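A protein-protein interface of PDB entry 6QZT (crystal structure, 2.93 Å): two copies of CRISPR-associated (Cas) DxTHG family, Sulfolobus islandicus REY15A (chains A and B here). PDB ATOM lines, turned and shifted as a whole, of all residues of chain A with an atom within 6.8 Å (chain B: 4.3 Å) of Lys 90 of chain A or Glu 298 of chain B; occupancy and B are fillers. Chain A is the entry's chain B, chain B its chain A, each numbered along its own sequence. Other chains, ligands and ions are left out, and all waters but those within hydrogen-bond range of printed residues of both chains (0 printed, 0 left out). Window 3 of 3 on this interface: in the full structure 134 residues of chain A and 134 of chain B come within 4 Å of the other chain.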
ATOM      1  N   LEU A  47      30.727 -11.483  18.821  1.00  0.00           N
ATOM      2  CA  LEU A  47      31.532 -10.228  18.713  1.00  0.00           C
ATOM      3  C   LEU A  47      31.822  -9.805  17.263  1.00  0.00           C
ATOM      4  O   LEU A  47      33.013  -9.629  16.948  1.00  0.00           O
ATOM      5  CB  LEU A  47      32.838 -10.428  19.487  1.00  0.00           C
ATOM      6  CG  LEU A  47      32.688 -11.090  20.854  1.00  0.00           C
ATOM      7  CD1 LEU A  47      34.025 -11.615  21.350  1.00  0.00           C
ATOM      8  CD2 LEU A  47      32.093 -10.120  21.861  1.00  0.00           C
ATOM      9  N   ILE A  48      30.798  -9.689  16.416  1.00  0.00           N
ATOM     10  CA  ILE A  48      30.994  -9.396  14.960  1.00  0.00           C
ATOM     11  C   ILE A  48      31.683  -8.046  14.722  1.00  0.00           C
ATOM     12  O   ILE A  48      31.075  -7.012  15.036  1.00  0.00           O
ATOM     13  CB  ILE A  48      29.654  -9.473  14.203  1.00  0.00           C
ATOM     14  CG1 ILE A  48      29.147 -10.912  14.090  1.00  0.00           C
ATOM     15  CG2 ILE A  48      29.775  -8.810  12.842  1.00  0.00           C
ATOM     16  CD1 ILE A  48      29.336 -11.728  15.346  1.00  0.00           C
ATOM     17  N   PRO A  49      32.907  -8.013  14.149  1.00  0.00           N
ATOM     18  CA  PRO A  49      33.591  -6.753  13.835  1.00  0.00           C
ATOM     19  C   PRO A  49      32.826  -6.052  12.702  1.00  0.00           C
ATOM     20  O   PRO A  49      32.346  -6.735  11.822  1.00  0.00           O
ATOM     21  CB  PRO A  49      34.975  -7.195  13.342  1.00  0.00           C
ATOM     22  CG  PRO A  49      34.766  -8.616  12.873  1.00  0.00           C
ATOM     23  CD  PRO A  49      33.706  -9.183  13.792  1.00  0.00           C
ATOM     24  N   ASP A  50      32.755  -4.718  12.741  1.00  0.00           N
ATOM     25  CA  ASP A  50      31.988  -3.933  11.733  1.00  0.00           C
ATOM     26  C   ASP A  50      32.516  -4.056  10.297  1.00  0.00           C
ATOM     27  O   ASP A  50      31.689  -4.092   9.376  1.00  0.00           O
ATOM     28  CB  ASP A  50      31.773  -2.478  12.176  1.00  0.00           C
ATOM     29  CG  ASP A  50      33.034  -1.639  12.307  1.00  0.00           C
ATOM     30  OD1 ASP A  50      34.106  -2.116  11.893  1.00  0.00           O
ATOM     31  OD2 ASP A  50      32.929  -0.506  12.812  1.00  0.00           O
ATOM     32  N   ASP A  59      22.841  -6.838   9.791  1.00  0.00           N
ATOM     33  CA  ASP A  59      23.949  -7.742   9.361  1.00  0.00           C
ATOM     34  C   ASP A  59      24.222  -8.909  10.344  1.00  0.00           C
ATOM     35  O   ASP A  59      24.717  -9.965   9.906  1.00  0.00           O
ATOM     36  CB  ASP A  59      25.265  -6.978   9.193  1.00  0.00           C
ATOM     37  CG  ASP A  59      25.747  -6.312  10.468  1.00  0.00           C
ATOM     38  OD1 ASP A  59      25.018  -6.378  11.477  1.00  0.00           O
ATOM     39  OD2 ASP A  59      26.850  -5.735  10.441  1.00  0.00           O
ATOM     40  N   GLU A  60      23.885  -8.701  11.621  1.00  0.00           N
ATOM     41  CA  GLU A  60      24.012  -9.751  12.665  1.00  0.00           C
ATOM     42  C   GLU A  60      23.592 -11.189  12.329  1.00  0.00           C
ATOM     43  O   GLU A  60      23.953 -12.093  13.103  1.00  0.00           O
ATOM     44  CB  GLU A  60      23.381  -9.397  14.013  1.00  0.00           C
ATOM     45  CG  GLU A  60      21.880  -9.199  13.943  1.00  0.00           C
ATOM     46  CD  GLU A  60      21.259  -8.730  15.247  1.00  0.00           C
ATOM     47  OE1 GLU A  60      21.915  -8.878  16.295  1.00  0.00           O
ATOM     48  OE2 GLU A  60      20.123  -8.218  15.211  1.00  0.00           O
ATOM     49  N   ILE A  88      25.156 -12.721  18.927  1.00  0.00           N
ATOM     50  CA  ILE A  88      26.050 -11.982  18.033  1.00  0.00           C
ATOM     51  C   ILE A  88      26.053 -10.534  18.490  1.00  0.00           C
ATOM     52  O   ILE A  88      24.986  -9.995  18.785  1.00  0.00           O
ATOM     53  CB  ILE A  88      25.610 -12.132  16.534  1.00  0.00           C
ATOM     54  CG1 ILE A  88      26.098 -13.452  15.899  1.00  0.00           C
ATOM     55  CG2 ILE A  88      26.043 -10.950  15.664  1.00  0.00           C
ATOM     56  CD1 ILE A  88      25.163 -14.637  16.008  1.00  0.00           C
ATOM     57  N   ARG A  89      27.238  -9.906  18.548  1.00  0.00           N
ATOM     58  CA  ARG A  89      27.367  -8.496  18.912  1.00  0.00           C
ATOM     59  C   ARG A  89      28.262  -7.692  17.993  1.00  0.00           C
ATOM     60  O   ARG A  89      29.370  -8.111  17.698  1.00  0.00           O
ATOM     61  CB  ARG A  89      27.784  -8.308  20.380  1.00  0.00           C
ATOM     62  CG  ARG A  89      26.642  -8.470  21.388  1.00  0.00           C
ATOM     63  CD  ARG A  89      25.961  -7.162  21.788  1.00  0.00           C
ATOM     64  NE  ARG A  89      24.902  -6.755  20.857  1.00  0.00           N
ATOM     65  CZ  ARG A  89      23.629  -7.134  20.945  1.00  0.00           C
ATOM     66  NH1 ARG A  89      23.236  -7.946  21.920  1.00  0.00           N
ATOM     67  NH2 ARG A  89      22.742  -6.715  20.052  1.00  0.00           N
ATOM     68  N   LYS A  90      27.766  -6.546  17.524  1.00  0.00           N
ATOM     69  CA  LYS A  90      28.502  -5.628  16.636  1.00  0.00           C
ATOM     70  C   LYS A  90      29.652  -4.867  17.321  1.00  0.00           C
ATOM     71  O   LYS A  90      29.408  -4.208  18.327  1.00  0.00           O
ATOM     72  CB  LYS A  90      27.512  -4.607  16.021  1.00  0.00           C
ATOM     73  CG  LYS A  90      26.836  -3.677  17.052  1.00  0.00           C
ATOM     74  CD  LYS A  90      25.858  -2.673  16.418  1.00  0.00           C
ATOM     75  CE  LYS A  90      25.204  -1.768  17.442  1.00  0.00           C
ATOM     76  NZ  LYS A  90      24.327  -2.518  18.383  1.00  0.00           N
ATOM     77  N   ILE A  91      30.904  -5.046  16.850  1.00  0.00           N
ATOM     78  CA  ILE A  91      32.107  -4.450  17.440  1.00  0.00           C
ATOM     79  C   ILE A  91      32.874  -3.566  16.441  1.00  0.00           C
ATOM     80  O   ILE A  91      32.992  -3.941  15.279  1.00  0.00           O
ATOM     81  CB  ILE A  91      33.055  -5.398  18.256  1.00  0.00           C
ATOM     82  CG1 ILE A  91      33.983  -6.254  17.364  1.00  0.00           C
ATOM     83  CG2 ILE A  91      32.283  -6.282  19.256  1.00  0.00           C
ATOM     84  CD1 ILE A  91      35.337  -6.566  18.022  1.00  0.00           C
ATOM     85  N   PRO A  92      33.406  -2.398  16.866  1.00  0.00           N
ATOM     86  CA  PRO A  92      34.130  -1.533  15.917  1.00  0.00           C
ATOM     87  C   PRO A  92      35.488  -2.063  15.473  1.00  0.00           C
ATOM     88  O   PRO A  92      35.926  -3.103  15.959  1.00  0.00           O
ATOM     89  CB  PRO A  92      34.241  -0.193  16.656  1.00  0.00           C
ATOM     90  CG  PRO A  92      34.122  -0.520  18.069  1.00  0.00           C
ATOM     91  CD  PRO A  92      33.342  -1.790  18.207  1.00  0.00           C
ATOM     92  N   PHE A 132      38.309   3.419  22.206  1.00  0.00           N
ATOM     93  CA  PHE A 132      36.900   3.430  21.791  1.00  0.00           C
ATOM     94  C   PHE A 132      36.482   1.974  21.585  1.00  0.00           C
ATOM     95  O   PHE A 132      35.510   1.518  22.197  1.00  0.00           O
ATOM     96  CB  PHE A 132      36.718   4.261  20.495  1.00  0.00           C
ATOM     97  CG  PHE A 132      35.380   4.150  19.792  1.00  0.00           C
ATOM     98  CD1 PHE A 132      34.292   4.910  20.206  1.00  0.00           C
ATOM     99  CD2 PHE A 132      35.213   3.299  18.704  1.00  0.00           C
ATOM    100  CE1 PHE A 132      33.058   4.816  19.550  1.00  0.00           C
ATOM    101  CE2 PHE A 132      33.970   3.187  18.063  1.00  0.00           C
ATOM    102  CZ  PHE A 132      32.901   3.946  18.493  1.00  0.00           C
ATOM    103  N   ALA A 136      33.867  -0.248  23.827  1.00  0.00           N
ATOM    104  CA  ALA A 136      32.789  -0.954  23.134  1.00  0.00           C
ATOM    105  C   ALA A 136      32.781  -2.444  23.468  1.00  0.00           C
ATOM    106  O   ALA A 136      31.727  -2.979  23.810  1.00  0.00           O
ATOM    107  CB  ALA A 136      32.924  -0.752  21.644  1.00  0.00           C
ATOM    108  N   ILE A 140      30.186  -4.832  26.122  1.00  0.00           N
ATOM    109  CA  ILE A 140      29.612  -6.135  25.755  1.00  0.00           C
ATOM    110  C   ILE A 140      29.895  -7.187  26.827  1.00  0.00           C
ATOM    111  O   ILE A 140      28.972  -7.861  27.299  1.00  0.00           O
ATOM    112  CB  ILE A 140      30.054  -6.579  24.324  1.00  0.00           C
ATOM    113  CG1 ILE A 140      29.641  -5.515  23.278  1.00  0.00           C
ATOM    114  CG2 ILE A 140      29.462  -7.964  23.963  1.00  0.00           C
ATOM    115  CD1 ILE A 140      30.497  -5.395  22.140  1.00  0.00           C
ATOM    116  N   LYS B 295      27.063   0.253  23.854  1.00  0.00           N
ATOM    117  CA  LYS B 295      26.353  -0.957  23.423  1.00  0.00           C
ATOM    118  C   LYS B 295      25.744  -0.667  22.047  1.00  0.00           C
ATOM    119  O   LYS B 295      25.632  -1.571  21.217  1.00  0.00           O
ATOM    120  CB  LYS B 295      25.229  -1.322  24.407  1.00  0.00           C
ATOM    121  CG  LYS B 295      25.676  -2.125  25.612  1.00  0.00           C
ATOM    122  CD  LYS B 295      24.477  -2.658  26.387  1.00  0.00           C
ATOM    123  CE  LYS B 295      24.227  -4.128  26.108  1.00  0.00           C
ATOM    124  NZ  LYS B 295      23.170  -4.695  26.984  1.00  0.00           N
ATOM    125  N   ASN B 296      25.350   0.608  21.826  1.00  0.00           N
ATOM    126  CA  ASN B 296      24.774   1.134  20.586  1.00  0.00           C
ATOM    127  C   ASN B 296      25.768   2.154  20.033  1.00  0.00           C
ATOM    128  O   ASN B 296      25.408   3.290  19.712  1.00  0.00           O
ATOM    129  CB  ASN B 296      23.391   1.759  20.860  1.00  0.00           C
ATOM    130  CG  ASN B 296      22.396   0.796  21.475  1.00  0.00           C
ATOM    131  OD1 ASN B 296      22.468   0.452  22.662  1.00  0.00           O
ATOM    132  ND2 ASN B 296      21.431   0.343  20.680  1.00  0.00           N
ATOM    133  N   TRP B 297      27.041   1.732  19.968  1.00  0.00           N
ATOM    134  CA  TRP B 297      28.204   2.505  19.536  1.00  0.00           C
ATOM    135  C   TRP B 297      28.152   3.094  18.135  1.00  0.00           C
ATOM    136  O   TRP B 297      28.761   4.141  17.896  1.00  0.00           O
ATOM    137  CB  TRP B 297      29.480   1.657  19.675  1.00  0.00           C
ATOM    138  CG  TRP B 297      29.470   0.388  18.867  1.00  0.00           C
ATOM    139  CD1 TRP B 297      28.999  -0.834  19.250  1.00  0.00           C
ATOM    140  CD2 TRP B 297      29.975   0.225  17.540  1.00  0.00           C
ATOM    141  NE1 TRP B 297      29.149  -1.740  18.228  1.00  0.00           N
ATOM    142  CE2 TRP B 297      29.763  -1.124  17.172  1.00  0.00           C
ATOM    143  CE3 TRP B 297      30.564   1.097  16.610  1.00  0.00           C
ATOM    144  CZ2 TRP B 297      30.101  -1.616  15.912  1.00  0.00           C
ATOM    145  CZ3 TRP B 297      30.895   0.609  15.358  1.00  0.00           C
ATOM    146  CH2 TRP B 297      30.673  -0.736  15.023  1.00  0.00           C
ATOM    147  N   GLU B 298      27.395   2.449  17.246  1.00  0.00           N
ATOM    148  CA  GLU B 298      27.278   2.905  15.835  1.00  0.00           C
ATOM    149  C   GLU B 298      26.425   4.179  15.722  1.00  0.00           C
ATOM    150  O   GLU B 298      26.716   5.004  14.837  1.00  0.00           O
ATOM    151  CB  GLU B 298      26.624   1.814  14.984  1.00  0.00           C
ATOM    152  CG  GLU B 298      27.483   0.575  14.818  1.00  0.00           C
ATOM    153  CD  GLU B 298      26.828  -0.552  14.037  1.00  0.00           C
ATOM    154  OE1 GLU B 298      25.615  -0.455  13.770  1.00  0.00           O
ATOM    155  OE2 GLU B 298      27.533  -1.522  13.696  1.00  0.00           O
ATOM    156  N   GLU B 299      25.451   4.352  16.619  1.00  0.00           N
ATOM    157  CA  GLU B 299      24.595   5.567  16.592  1.00  0.00           C
ATOM    158  C   GLU B 299      25.549   6.662  17.083  1.00  0.00           C
ATOM    159  O   GLU B 299      25.587   7.738  16.456  1.00  0.00           O
ATOM    160  CB  GLU B 299      23.428   5.425  17.569  1.00  0.00           C
ATOM    161  CG  GLU B 299      22.183   4.833  16.937  1.00  0.00           C
ATOM    162  CD  GLU B 299      21.577   3.671  17.705  1.00  0.00           C
ATOM    163  OE1 GLU B 299      21.795   3.600  18.928  1.00  0.00           O
ATOM    164  OE2 GLU B 299      20.890   2.842  17.078  1.00  0.00           O
ATOM    165  N   HIS B 300      26.297   6.388  18.156  1.00  0.00           N
ATOM    166  CA  HIS B 300      27.334   7.356  18.631  1.00  0.00           C
ATOM    167  C   HIS B 300      28.822   7.272  18.210  1.00  0.00           C
ATOM    168  O   HIS B 300      29.618   6.611  18.897  1.00  0.00           O
ATOM    169  CB  HIS B 300      27.300   7.305  20.163  1.00  0.00           C
ATOM    170  CG  HIS B 300      25.954   7.586  20.737  1.00  0.00           C
ATOM    171  ND1 HIS B 300      25.373   8.836  20.677  1.00  0.00           N
ATOM    172  CD2 HIS B 300      25.073   6.789  21.378  1.00  0.00           C
ATOM    173  CE1 HIS B 300      24.190   8.796  21.257  1.00  0.00           C
ATOM    174  NE2 HIS B 300      23.984   7.552  21.696  1.00  0.00           N
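Lys 90 of chain A touches just these residues of chain B: Lys 295, Trp 297 and Glu 298. Of chain A, only Lys 90 comes within 4 Å of Glu 298 of chain B. Of the printed residues of chain B, Pro 92 of chain A touches Trp 297. Of the printed residues of chain B, Ile 91 of chain A touches Trp 297 (3.4 Å). Printed residues of chain A within 4 Å of Trp 297 of chain B: Asp 50 (3.2 Å), Lys 90 (2.5 Å), Ile 91 (3.4 Å) and Pro 92 (3.5 Å). The nearest printed residue of chain B that does not touch Lys 90 of chain A is Asn 296 of chain B (4.3 Å). The nearest printed residue of chain A that does not touch Lys 295 of chain B is Arg 89 of chain A (5.2 Å).
Asp 50 of chain A touches Trp 297 of chain B (OD2 to CH2, 3.2 Å). Glu 298 of chain B touches Lys 90 of chain A (CD to CD, 3.3 Å). Ile 91 of chain A touches Trp 297 of chain B (C to CZ2, 3.4 Å). N of Pro 92 of chain A touches CZ2 of Trp 297 of chain B (3.5 Å). CE1 of Phe 132 of chain A touches O of His 300 of chain B, 3.9 Å away.
The side-chain amino group of Lys 90 of chain A lies within hydrogen-bond range of the backbone carbonyl oxygen of Lys 295 of chain B, 3.3 Å away. O of Lys 90 of chain A lies within hydrogen-bond range of NE1 of Trp 297 of chain B, at 2.5 Å.
No position is printed for both chains.
O of Ile 48 of chain A is in hydrogen-bond range of N of Ile 91 of chain A, 2.7 Å away. O of Ile 91 of chain A is in hydrogen-bond range of N of Asp 50 of chain A, 2.7 Å away.
Printed residues of chain A that touch a printed residue of chain B: Asp 50, Lys 90, Ile 91, Pro 92 and Phe 132. Hydrophobic or aromatic side chains of chain A within 4 Å of the printed part of chain B: Pro 92 and Phe 132. Hydrophobic or aromatic side chains of chain B that line the printed part of chain A: Trp 297. Among the printed residues, no Asp or Glu carboxylate lies within 4 Å of a Lys or Arg side-chain nitrogen of the other chain.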
